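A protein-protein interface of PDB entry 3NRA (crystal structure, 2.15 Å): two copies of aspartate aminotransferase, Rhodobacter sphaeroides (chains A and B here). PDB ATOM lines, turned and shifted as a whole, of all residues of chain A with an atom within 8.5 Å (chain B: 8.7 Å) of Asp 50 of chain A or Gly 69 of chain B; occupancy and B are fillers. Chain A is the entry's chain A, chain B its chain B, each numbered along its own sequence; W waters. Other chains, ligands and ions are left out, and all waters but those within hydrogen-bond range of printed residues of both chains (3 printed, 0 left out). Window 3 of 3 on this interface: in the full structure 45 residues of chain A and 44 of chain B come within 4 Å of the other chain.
The side-chain carboxylate (OD1) of Asp 50 of chain A is in hydrogen-bond range of the backbone NH (N) of Gly 70 of chain B (2.9 Å).
The backbone carbonyl oxygen (O) of Gly 259 of chain A lies within hydrogen-bond range of the backbone NH (N) of Gly 288 of chain B, 3.3 Å away.
O of Gly 259 of chain A is in hydrogen-bond range of N of Tyr 289 of chain B, at 3.2 Å.
The backbone carbonyl oxygen (O) of His 46 of chain A is in hydrogen-bond range of the side-chain amide nitrogen (NE2) of Gln 386 of chain A, 3.0 Å away.
N of Asp 50 of chain A lies within hydrogen-bond range of OD1 of Asp 48 of chain A.
The side-chain amide nitrogen (NE2) of Gln 72 of chain B sits at hydrogen-bond distance from the backbone carbonyl oxygen (O) of Gly 288 of chain B (2.9 Å).
ND1 of His 46 of chain A touches CG of Tyr 74 of chain B, at 3.5 Å.
Gly 47 of chain A touches Tyr 74 of chain B (O to CE1, 3.97 Å).
Val 49 of chain A touches Gly 70 of chain B.
Asp 50 of chain A touches Gly 69 of chain B.
Tyr 289 of chain B touches Pro 54 of chain A (OH to CG, 3.8 Å).
Gly 259 of chain A touches Ala 73 of chain B (CA to O, 3.7 Å).
Of chain B, only Gly 69 (3.3 Å) and Gly 70 (2.9 Å) come within 4 Å of Asp 50 of chain A.
Of chain A, only Asp 50 comes within 4 Å of Gly 69 of chain B.
No residue of chain B comes within 4 Å of Ala 51 of chain A.
Ser 68 of chain B touches none of the printed residues of chain A.
Gly 70 of chain B touches just these residues of chain A: Val 49 and Asp 50.
Printed residues of chain B within 4 Å of Pro 54 of chain A: Tyr 289 (3.8 Å).
Printed residues of chain B within 4 Å of Gly 259 of chain A: Ala 73 (3.7 Å), Gly 288 (3.3 Å) and Tyr 289 (3.2 Å).
Of the printed residues of chain B, Gly 47 of chain A touches Tyr 74.
Gln 67 of chain B touches none of the printed residues of chain A.
Ala 64 of chain B touches none of the printed residues of chain A.
The nearest residue of chain B that does not touch Asp 50 of chain A is Ser 68 of chain B (4.2 Å).
Hydrophobic or aromatic side chains of chain B within 4 Å of the printed part of chain A: Tyr 74 and Tyr 289.
Of the 15 printed residues of chain A, 6 touch a printed residue of chain B.
Hydrophobic or aromatic side chains of chain A that line the printed part of chain B: His 46, Val 49 and Pro 54.
Among the printed residues, 9 pairs touch across the chains.
Among the printed residues, no Asp or Glu carboxylate lies within 4 Å of a Lys or Arg side-chain nitrogen of the other chain.
No position is printed for both chains.
Of the 9 pairs that touch across the chains among the printed residues, none has its exchanged pair printed and touching as well.
Water W1 lies within hydrogen-bond range of O of Ser 68 of chain B (2.5 Å), N of Val 71 of chain B (2.9 Å), OD2 of Asp 50 of chain A (3.0 Å) and N of Gly 70 of chain B (3.0 Å).
Water W3 lies within hydrogen-bond range of the side-chain hydroxyl of Tyr 289 of chain B, the backbone carbonyl oxygen of Ser 256 of chain A and the backbone NH of Gly 259 of chain A.
Water W2 bridges OH of Tyr 74 of chain B and N of Gly 47 of chain A.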
ATOM      1  N   HIS A  46       0.532 -33.520  14.644  1.00  0.00           N
ATOM      2  CA  HIS A  46       1.616 -33.206  13.716  1.00  0.00           C
ATOM      3  C   HIS A  46       2.698 -32.443  14.445  1.00  0.00           C
ATOM      4  O   HIS A  46       2.552 -32.134  15.602  1.00  0.00           O
ATOM      5  CB  HIS A  46       1.090 -32.400  12.530  1.00  0.00           C
ATOM      6  CG  HIS A  46       0.492 -31.088  12.917  1.00  0.00           C
ATOM      7  ND1 HIS A  46       1.236 -29.931  13.017  1.00  0.00           N
ATOM      8  CD2 HIS A  46      -0.762 -30.757  13.266  1.00  0.00           C
ATOM      9  CE1 HIS A  46       0.452 -28.939  13.386  1.00  0.00           C
ATOM     10  NE2 HIS A  46      -0.764 -29.414  13.553  1.00  0.00           N
ATOM     11  N   GLY A  47       3.807 -32.200  13.778  1.00  0.00           N
ATOM     12  CA  GLY A  47       4.945 -31.534  14.412  1.00  0.00           C
ATOM     13  C   GLY A  47       4.723 -30.056  14.659  1.00  0.00           C
ATOM     14  O   GLY A  47       3.846 -29.436  14.059  1.00  0.00           O
ATOM     15  N   ASP A  48       5.500 -29.512  15.594  1.00  0.00           N
ATOM     16  CA  ASP A  48       5.397 -28.145  15.996  1.00  0.00           C
ATOM     17  C   ASP A  48       6.580 -27.450  15.372  1.00  0.00           C
ATOM     18  O   ASP A  48       7.718 -27.640  15.812  1.00  0.00           O
ATOM     19  CB  ASP A  48       5.457 -28.052  17.515  1.00  0.00           C
ATOM     20  CG  ASP A  48       5.321 -26.620  18.036  1.00  0.00           C
ATOM     21  OD1 ASP A  48       5.540 -25.666  17.275  1.00  0.00           O
ATOM     22  OD2 ASP A  48       4.987 -26.462  19.226  1.00  0.00           O
ATOM     23  N   VAL A  49       6.343 -26.674  14.320  1.00  0.00           N
ATOM     24  CA  VAL A  49       7.455 -25.975  13.657  1.00  0.00           C
ATOM     25  C   VAL A  49       7.770 -24.594  14.254  1.00  0.00           C
ATOM     26  O   VAL A  49       8.597 -23.860  13.687  1.00  0.00           O
ATOM     27  CB  VAL A  49       7.250 -25.849  12.139  1.00  0.00           C
ATOM     28  CG1 VAL A  49       6.831 -27.198  11.553  1.00  0.00           C
ATOM     29  CG2 VAL A  49       6.255 -24.741  11.819  1.00  0.00           C
ATOM     30  N   ASP A  50       7.123 -24.237  15.381  1.00  0.00           N
ATOM     31  CA  ASP A  50       7.585 -23.114  16.226  1.00  0.00           C
ATOM     32  C   ASP A  50       8.638 -23.614  17.220  1.00  0.00           C
ATOM     33  O   ASP A  50       9.619 -22.906  17.520  1.00  0.00           O
ATOM     34  CB  ASP A  50       6.425 -22.458  16.997  1.00  0.00           C
ATOM     35  CG  ASP A  50       5.282 -22.013  16.090  1.00  0.00           C
ATOM     36  OD1 ASP A  50       5.548 -21.630  14.945  1.00  0.00           O
ATOM     37  OD2 ASP A  50       4.118 -22.056  16.534  1.00  0.00           O
ATOM     38  N   ALA A  51       8.445 -24.837  17.707  1.00  0.00           N
ATOM     39  CA  ALA A  51       9.388 -25.473  18.615  1.00  0.00           C
ATOM     40  C   ALA A  51      10.661 -25.976  17.871  1.00  0.00           C
ATOM     41  O   ALA A  51      11.755 -25.973  18.435  1.00  0.00           O
ATOM     42  CB  ALA A  51       8.723 -26.599  19.312  1.00  0.00           C
ATOM     43  N   HIS A  52      10.484 -26.491  16.643  1.00  0.00           N
ATOM     44  CA  HIS A  52      11.605 -26.941  15.821  1.00  0.00           C
ATOM     45  C   HIS A  52      11.462 -26.278  14.476  1.00  0.00           C
ATOM     46  O   HIS A  52      10.653 -26.702  13.628  1.00  0.00           O
ATOM     47  CB  HIS A  52      11.624 -28.463  15.737  1.00  0.00           C
ATOM     48  CG  HIS A  52      11.563 -29.123  17.078  1.00  0.00           C
ATOM     49  ND1 HIS A  52      12.683 -29.324  17.858  1.00  0.00           N
ATOM     50  CD2 HIS A  52      10.508 -29.561  17.811  1.00  0.00           C
ATOM     51  CE1 HIS A  52      12.323 -29.886  19.001  1.00  0.00           C
ATOM     52  NE2 HIS A  52      11.006 -30.020  19.005  1.00  0.00           N
ATOM     53  N   GLU A  53      12.220 -25.189  14.318  1.00  0.00           N
ATOM     54  CA  GLU A  53      12.044 -24.214  13.233  1.00  0.00           C
ATOM     55  C   GLU A  53      12.393 -24.777  11.860  1.00  0.00           C
ATOM     56  O   GLU A  53      13.209 -25.692  11.760  1.00  0.00           O
ATOM     57  CB  GLU A  53      12.907 -22.961  13.492  1.00  0.00           C
ATOM     58  CG  GLU A  53      14.461 -23.180  13.446  1.00  0.00           C
ATOM     59  CD  GLU A  53      15.249 -21.908  13.793  1.00  0.00           C
ATOM     60  OE1 GLU A  53      14.612 -20.917  14.167  1.00  0.00           O
ATOM     61  OE2 GLU A  53      16.493 -21.906  13.673  1.00  0.00           O
ATOM     62  N   PRO A  54      11.800 -24.209  10.785  1.00  0.00           N
ATOM     63  CA  PRO A  54      12.246 -24.537   9.460  1.00  0.00           C
ATOM     64  C   PRO A  54      13.748 -24.285   9.305  1.00  0.00           C
ATOM     65  O   PRO A  54      14.298 -23.393   9.967  1.00  0.00           O
ATOM     66  CB  PRO A  54      11.440 -23.562   8.584  1.00  0.00           C
ATOM     67  CG  PRO A  54      10.187 -23.311   9.328  1.00  0.00           C
ATOM     68  CD  PRO A  54      10.570 -23.351  10.758  1.00  0.00           C
ATOM     69  N   SER A 256      11.281 -29.404   8.963  1.00  0.00           N
ATOM     70  CA  SER A 256      10.187 -28.520   9.337  1.00  0.00           C
ATOM     71  C   SER A 256       9.787 -27.563   8.212  1.00  0.00           C
ATOM     72  O   SER A 256       9.376 -26.401   8.467  1.00  0.00           O
ATOM     73  CB  SER A 256      10.505 -27.777  10.662  1.00  0.00           C
ATOM     74  OG  SER A 256      10.670 -28.727  11.712  1.00  0.00           O
ATOM     75  N   GLY A 259       5.243 -26.371   5.393  1.00  0.00           N
ATOM     76  CA  GLY A 259       4.478 -25.243   4.849  1.00  0.00           C
ATOM     77  C   GLY A 259       4.831 -24.831   3.424  1.00  0.00           C
ATOM     78  O   GLY A 259       4.015 -24.203   2.750  1.00  0.00           O
ATOM     79  N   ARG A 308      19.644 -31.258  15.942  1.00  0.00           N
ATOM     80  CA  ARG A 308      18.219 -31.529  15.855  1.00  0.00           C
ATOM     81  C   ARG A 308      17.905 -32.979  16.276  1.00  0.00           C
ATOM     82  O   ARG A 308      16.974 -33.209  17.042  1.00  0.00           O
ATOM     83  CB  ARG A 308      17.704 -31.261  14.451  1.00  0.00           C
ATOM     84  CG  ARG A 308      16.256 -31.640  14.250  1.00  0.00           C
ATOM     85  CD  ARG A 308      15.569 -30.812  13.173  1.00  0.00           C
ATOM     86  NE  ARG A 308      15.407 -29.433  13.594  1.00  0.00           N
ATOM     87  CZ  ARG A 308      14.650 -28.516  12.982  1.00  0.00           C
ATOM     88  NH1 ARG A 308      13.959 -28.809  11.901  1.00  0.00           N
ATOM     89  NH2 ARG A 308      14.615 -27.264  13.470  1.00  0.00           N
ATOM     90  N   SER A 385       7.692 -34.184  17.885  1.00  0.00           N
ATOM     91  CA  SER A 385       8.446 -33.022  17.485  1.00  0.00           C
ATOM     92  C   SER A 385       7.737 -31.767  18.056  1.00  0.00           C
ATOM     93  O   SER A 385       6.965 -31.087  17.363  1.00  0.00           O
ATOM     94  CB  SER A 385       8.590 -32.968  15.960  1.00  0.00           C
ATOM     95  OG  SER A 385       9.494 -31.967  15.561  1.00  0.00           O
ATOM     96  N   GLN A 386       7.987 -31.524  19.352  1.00  0.00           N
ATOM     97  CA  GLN A 386       7.194 -30.620  20.166  1.00  0.00           C
ATOM     98  C   GLN A 386       8.141 -29.798  21.070  1.00  0.00           C
ATOM     99  O   GLN A 386       9.369 -30.055  21.118  1.00  0.00           O
ATOM    100  CB  GLN A 386       6.232 -31.419  21.055  1.00  0.00           C
ATOM    101  CG  GLN A 386       5.245 -32.351  20.304  1.00  0.00           C
ATOM    102  CD  GLN A 386       4.279 -31.620  19.419  1.00  0.00           C
ATOM    103  OE1 GLN A 386       3.946 -30.469  19.675  1.00  0.00           O
ATOM    104  NE2 GLN A 386       3.816 -32.288  18.346  1.00  0.00           N
ATOM    105  N   ASP A 387       7.578 -28.854  21.821  1.00  0.00           N
ATOM    106  CA  ASP A 387       8.312 -28.260  22.938  1.00  0.00           C
ATOM    107  C   ASP A 387       8.619 -29.384  23.937  1.00  0.00           C
ATOM    108  O   ASP A 387       7.721 -30.137  24.315  1.00  0.00           O
ATOM    109  CB  ASP A 387       7.493 -27.154  23.582  1.00  0.00           C
ATOM    110  CG  ASP A 387       8.161 -26.560  24.794  1.00  0.00           C
ATOM    111  OD1 ASP A 387       9.084 -25.731  24.630  1.00  0.00           O
ATOM    112  OD2 ASP A 387       7.757 -26.904  25.920  1.00  0.00           O
ATOM    113  N   PHE B  62       2.938 -13.384   2.534  1.00  0.00           N
ATOM    114  CA  PHE B  62       3.618 -14.677   2.620  1.00  0.00           C
ATOM    115  C   PHE B  62       4.616 -14.647   3.788  1.00  0.00           C
ATOM    116  O   PHE B  62       4.678 -15.578   4.616  1.00  0.00           O
ATOM    117  CB  PHE B  62       4.349 -15.001   1.287  1.00  0.00           C
ATOM    118  CG  PHE B  62       4.979 -16.370   1.267  1.00  0.00           C
ATOM    119  CD1 PHE B  62       6.253 -16.577   1.828  1.00  0.00           C
ATOM    120  CD2 PHE B  62       4.281 -17.453   0.789  1.00  0.00           C
ATOM    121  CE1 PHE B  62       6.802 -17.826   1.899  1.00  0.00           C
ATOM    122  CE2 PHE B  62       4.840 -18.721   0.806  1.00  0.00           C
ATOM    123  CZ  PHE B  62       6.110 -18.910   1.377  1.00  0.00           C
ATOM    124  N   SER B  63       5.361 -13.550   3.861  1.00  0.00           N
ATOM    125  CA  SER B  63       6.359 -13.353   4.887  1.00  0.00           C
ATOM    126  C   SER B  63       5.763 -13.226   6.311  1.00  0.00           C
ATOM    127  O   SER B  63       6.309 -13.756   7.260  1.00  0.00           O
ATOM    128  CB  SER B  63       7.175 -12.106   4.566  1.00  0.00           C
ATOM    129  OG  SER B  63       8.147 -11.939   5.561  1.00  0.00           O
ATOM    130  N   ALA B  64       4.637 -12.536   6.435  1.00  0.00           N
ATOM    131  CA  ALA B  64       3.910 -12.476   7.701  1.00  0.00           C
ATOM    132  C   ALA B  64       3.420 -13.880   8.133  1.00  0.00           C
ATOM    133  O   ALA B  64       3.477 -14.222   9.320  1.00  0.00           O
ATOM    134  CB  ALA B  64       2.739 -11.488   7.601  1.00  0.00           C
ATOM    135  N   GLY B  65       3.002 -14.696   7.167  1.00  0.00           N
ATOM    136  CA  GLY B  65       2.526 -16.080   7.454  1.00  0.00           C
ATOM    137  C   GLY B  65       3.649 -16.993   7.949  1.00  0.00           C
ATOM    138  O   GLY B  65       3.506 -17.692   8.955  1.00  0.00           O
ATOM    139  N   VAL B  66       4.785 -16.940   7.280  1.00  0.00           N
ATOM    140  CA  VAL B  66       5.931 -17.700   7.728  1.00  0.00           C
ATOM    141  C   VAL B  66       6.316 -17.327   9.167  1.00  0.00           C
ATOM    142  O   VAL B  66       6.423 -18.204  10.024  1.00  0.00           O
ATOM    143  CB  VAL B  66       7.113 -17.522   6.811  1.00  0.00           C
ATOM    144  CG1 VAL B  66       8.356 -18.164   7.434  1.00  0.00           C
ATOM    145  CG2 VAL B  66       6.796 -18.157   5.429  1.00  0.00           C
ATOM    146  N   GLN B  67       6.443 -16.028   9.433  1.00  0.00           N
ATOM    147  CA  GLN B  67       6.725 -15.529  10.785  1.00  0.00           C
ATOM    148  C   GLN B  67       5.681 -16.012  11.821  1.00  0.00           C
ATOM    149  O   GLN B  67       6.032 -16.298  12.950  1.00  0.00           O
ATOM    150  CB  GLN B  67       6.801 -13.986  10.772  1.00  0.00           C
ATOM    151  CG  GLN B  67       7.126 -13.316  12.138  1.00  0.00           C
ATOM    152  CD  GLN B  67       8.477 -13.766  12.710  1.00  0.00           C
ATOM    153  OE1 GLN B  67       9.412 -14.082  11.952  1.00  0.00           O
ATOM    154  NE2 GLN B  67       8.576 -13.829  14.048  1.00  0.00           N
ATOM    155  N   SER B  68       4.420 -16.097  11.428  1.00  0.00           N
ATOM    156  CA  SER B  68       3.355 -16.569  12.349  1.00  0.00           C
ATOM    157  C   SER B  68       3.515 -18.056  12.722  1.00  0.00           C
ATOM    158  O   SER B  68       3.057 -18.486  13.786  1.00  0.00           O
ATOM    159  CB  SER B  68       1.945 -16.325  11.752  1.00  0.00           C
ATOM    160  OG  SER B  68       1.644 -17.273  10.763  1.00  0.00           O
ATOM    161  N   GLY B  69       4.105 -18.825  11.815  1.00  0.00           N
ATOM    162  CA  GLY B  69       4.677 -20.115  12.130  1.00  0.00           C
ATOM    163  C   GLY B  69       3.716 -21.266  11.847  1.00  0.00           C
ATOM    164  O   GLY B  69       3.049 -21.308  10.785  1.00  0.00           O
ATOM    165  N   GLY B  70       3.607 -22.168  12.814  1.00  0.00           N
ATOM    166  CA  GLY B  70       2.926 -23.441  12.625  1.00  0.00           C
ATOM    167  C   GLY B  70       1.460 -23.314  12.339  1.00  0.00           C
ATOM    168  O   GLY B  70       0.902 -24.126  11.616  1.00  0.00           O
ATOM    169  N   VAL B  71       0.838 -22.263  12.873  1.00  0.00           N
ATOM    170  CA  VAL B  71      -0.568 -21.948  12.550  1.00  0.00           C
ATOM    171  C   VAL B  71      -0.795 -21.697  11.042  1.00  0.00           C
ATOM    172  O   VAL B  71      -1.872 -21.982  10.520  1.00  0.00           O
ATOM    173  CB  VAL B  71      -1.078 -20.729  13.381  1.00  0.00           C
ATOM    174  CG1 VAL B  71      -0.600 -19.450  12.783  1.00  0.00           C
ATOM    175  CG2 VAL B  71      -2.605 -20.759  13.495  1.00  0.00           C
ATOM    176  N   GLN B  72       0.230 -21.203  10.337  1.00  0.00           N
ATOM    177  CA  GLN B  72       0.119 -21.006   8.878  1.00  0.00           C
ATOM    178  C   GLN B  72       0.603 -22.239   8.097  1.00  0.00           C
ATOM    179  O   GLN B  72       0.055 -22.550   7.056  1.00  0.00           O
ATOM    180  CB  GLN B  72       0.874 -19.763   8.417  1.00  0.00           C
ATOM    181  CG  GLN B  72       0.547 -19.339   6.971  1.00  0.00           C
ATOM    182  CD  GLN B  72      -0.905 -18.936   6.807  1.00  0.00           C
ATOM    183  OE1 GLN B  72      -1.352 -17.967   7.403  1.00  0.00           O
ATOM    184  NE2 GLN B  72      -1.654 -19.704   6.018  1.00  0.00           N
ATOM    185  N   ALA B  73       1.640 -22.899   8.611  1.00  0.00           N
ATOM    186  CA  ALA B  73       2.280 -24.019   7.930  1.00  0.00           C
ATOM    187  C   ALA B  73       1.339 -25.192   7.811  1.00  0.00           C
ATOM    188  O   ALA B  73       1.386 -25.912   6.805  1.00  0.00           O
ATOM    189  CB  ALA B  73       3.544 -24.450   8.685  1.00  0.00           C
ATOM    190  N   TYR B  74       0.505 -25.402   8.857  1.00  0.00           N
ATOM    191  CA  TYR B  74      -0.504 -26.462   8.859  1.00  0.00           C
ATOM    192  C   TYR B  74      -1.938 -25.881   8.852  1.00  0.00           C
ATOM    193  O   TYR B  74      -2.256 -24.940   9.603  1.00  0.00           O
ATOM    194  CB  TYR B  74      -0.300 -27.389  10.071  1.00  0.00           C
ATOM    195  CG  TYR B  74       0.933 -28.267   9.950  1.00  0.00           C
ATOM    196  CD1 TYR B  74       2.193 -27.800  10.332  1.00  0.00           C
ATOM    197  CD2 TYR B  74       0.839 -29.555   9.454  1.00  0.00           C
ATOM    198  CE1 TYR B  74       3.339 -28.620  10.204  1.00  0.00           C
ATOM    199  CE2 TYR B  74       1.935 -30.361   9.335  1.00  0.00           C
ATOM    200  CZ  TYR B  74       3.188 -29.903   9.725  1.00  0.00           C
ATOM    201  OH  TYR B  74       4.266 -30.736   9.579  1.00  0.00           O
ATOM    202  N   THR B  75      -2.770 -26.400   7.963  1.00  0.00           N
ATOM    203  CA  THR B  75      -4.176 -25.957   7.816  1.00  0.00           C
ATOM    204  C   THR B  75      -5.015 -27.188   7.628  1.00  0.00           C
ATOM    205  O   THR B  75      -4.472 -28.282   7.351  1.00  0.00           O
ATOM    206  CB  THR B  75      -4.395 -25.087   6.537  1.00  0.00           C
ATOM    207  OG1 THR B  75      -4.377 -25.933   5.366  1.00  0.00           O
ATOM    208  CG2 THR B  75      -3.332 -23.974   6.404  1.00  0.00           C
ATOM    209  N   GLY B 288       0.706 -24.464   2.941  1.00  0.00           N
ATOM    210  CA  GLY B 288       0.287 -23.661   4.071  1.00  0.00           C
ATOM    211  C   GLY B 288       0.710 -22.205   3.968  1.00  0.00           C
ATOM    212  O   GLY B 288      -0.118 -21.314   4.098  1.00  0.00           O
ATOM    213  N   TYR B 289       1.991 -21.971   3.705  1.00  0.00           N
ATOM    214  CA  TYR B 289       2.508 -20.616   3.650  1.00  0.00           C
ATOM    215  C   TYR B 289       1.943 -19.856   2.465  1.00  0.00           C
ATOM    216  O   TYR B 289       1.586 -18.674   2.593  1.00  0.00           O
ATOM    217  CB  TYR B 289       4.036 -20.598   3.601  1.00  0.00           C
ATOM    218  CG  TYR B 289       4.735 -21.141   4.861  1.00  0.00           C
ATOM    219  CD1 TYR B 289       4.304 -20.807   6.128  1.00  0.00           C
ATOM    220  CD2 TYR B 289       5.859 -21.945   4.757  1.00  0.00           C
ATOM    221  CE1 TYR B 289       4.936 -21.300   7.246  1.00  0.00           C
ATOM    222  CE2 TYR B 289       6.517 -22.420   5.884  1.00  0.00           C
ATOM    223  CZ  TYR B 289       6.044 -22.119   7.109  1.00  0.00           C
ATOM    224  OH  TYR B 289       6.675 -22.597   8.219  1.00  0.00           O
HETATM  225  O   HOH W   1       2.146 -20.574  14.874  1.00  0.00           O
HETATM  226  O   HOH W   2       4.405 -33.170  11.025  1.00  0.00           O
HETATM  227  O   HOH W   3       6.995 -25.186   7.732  1.00  0.00           O
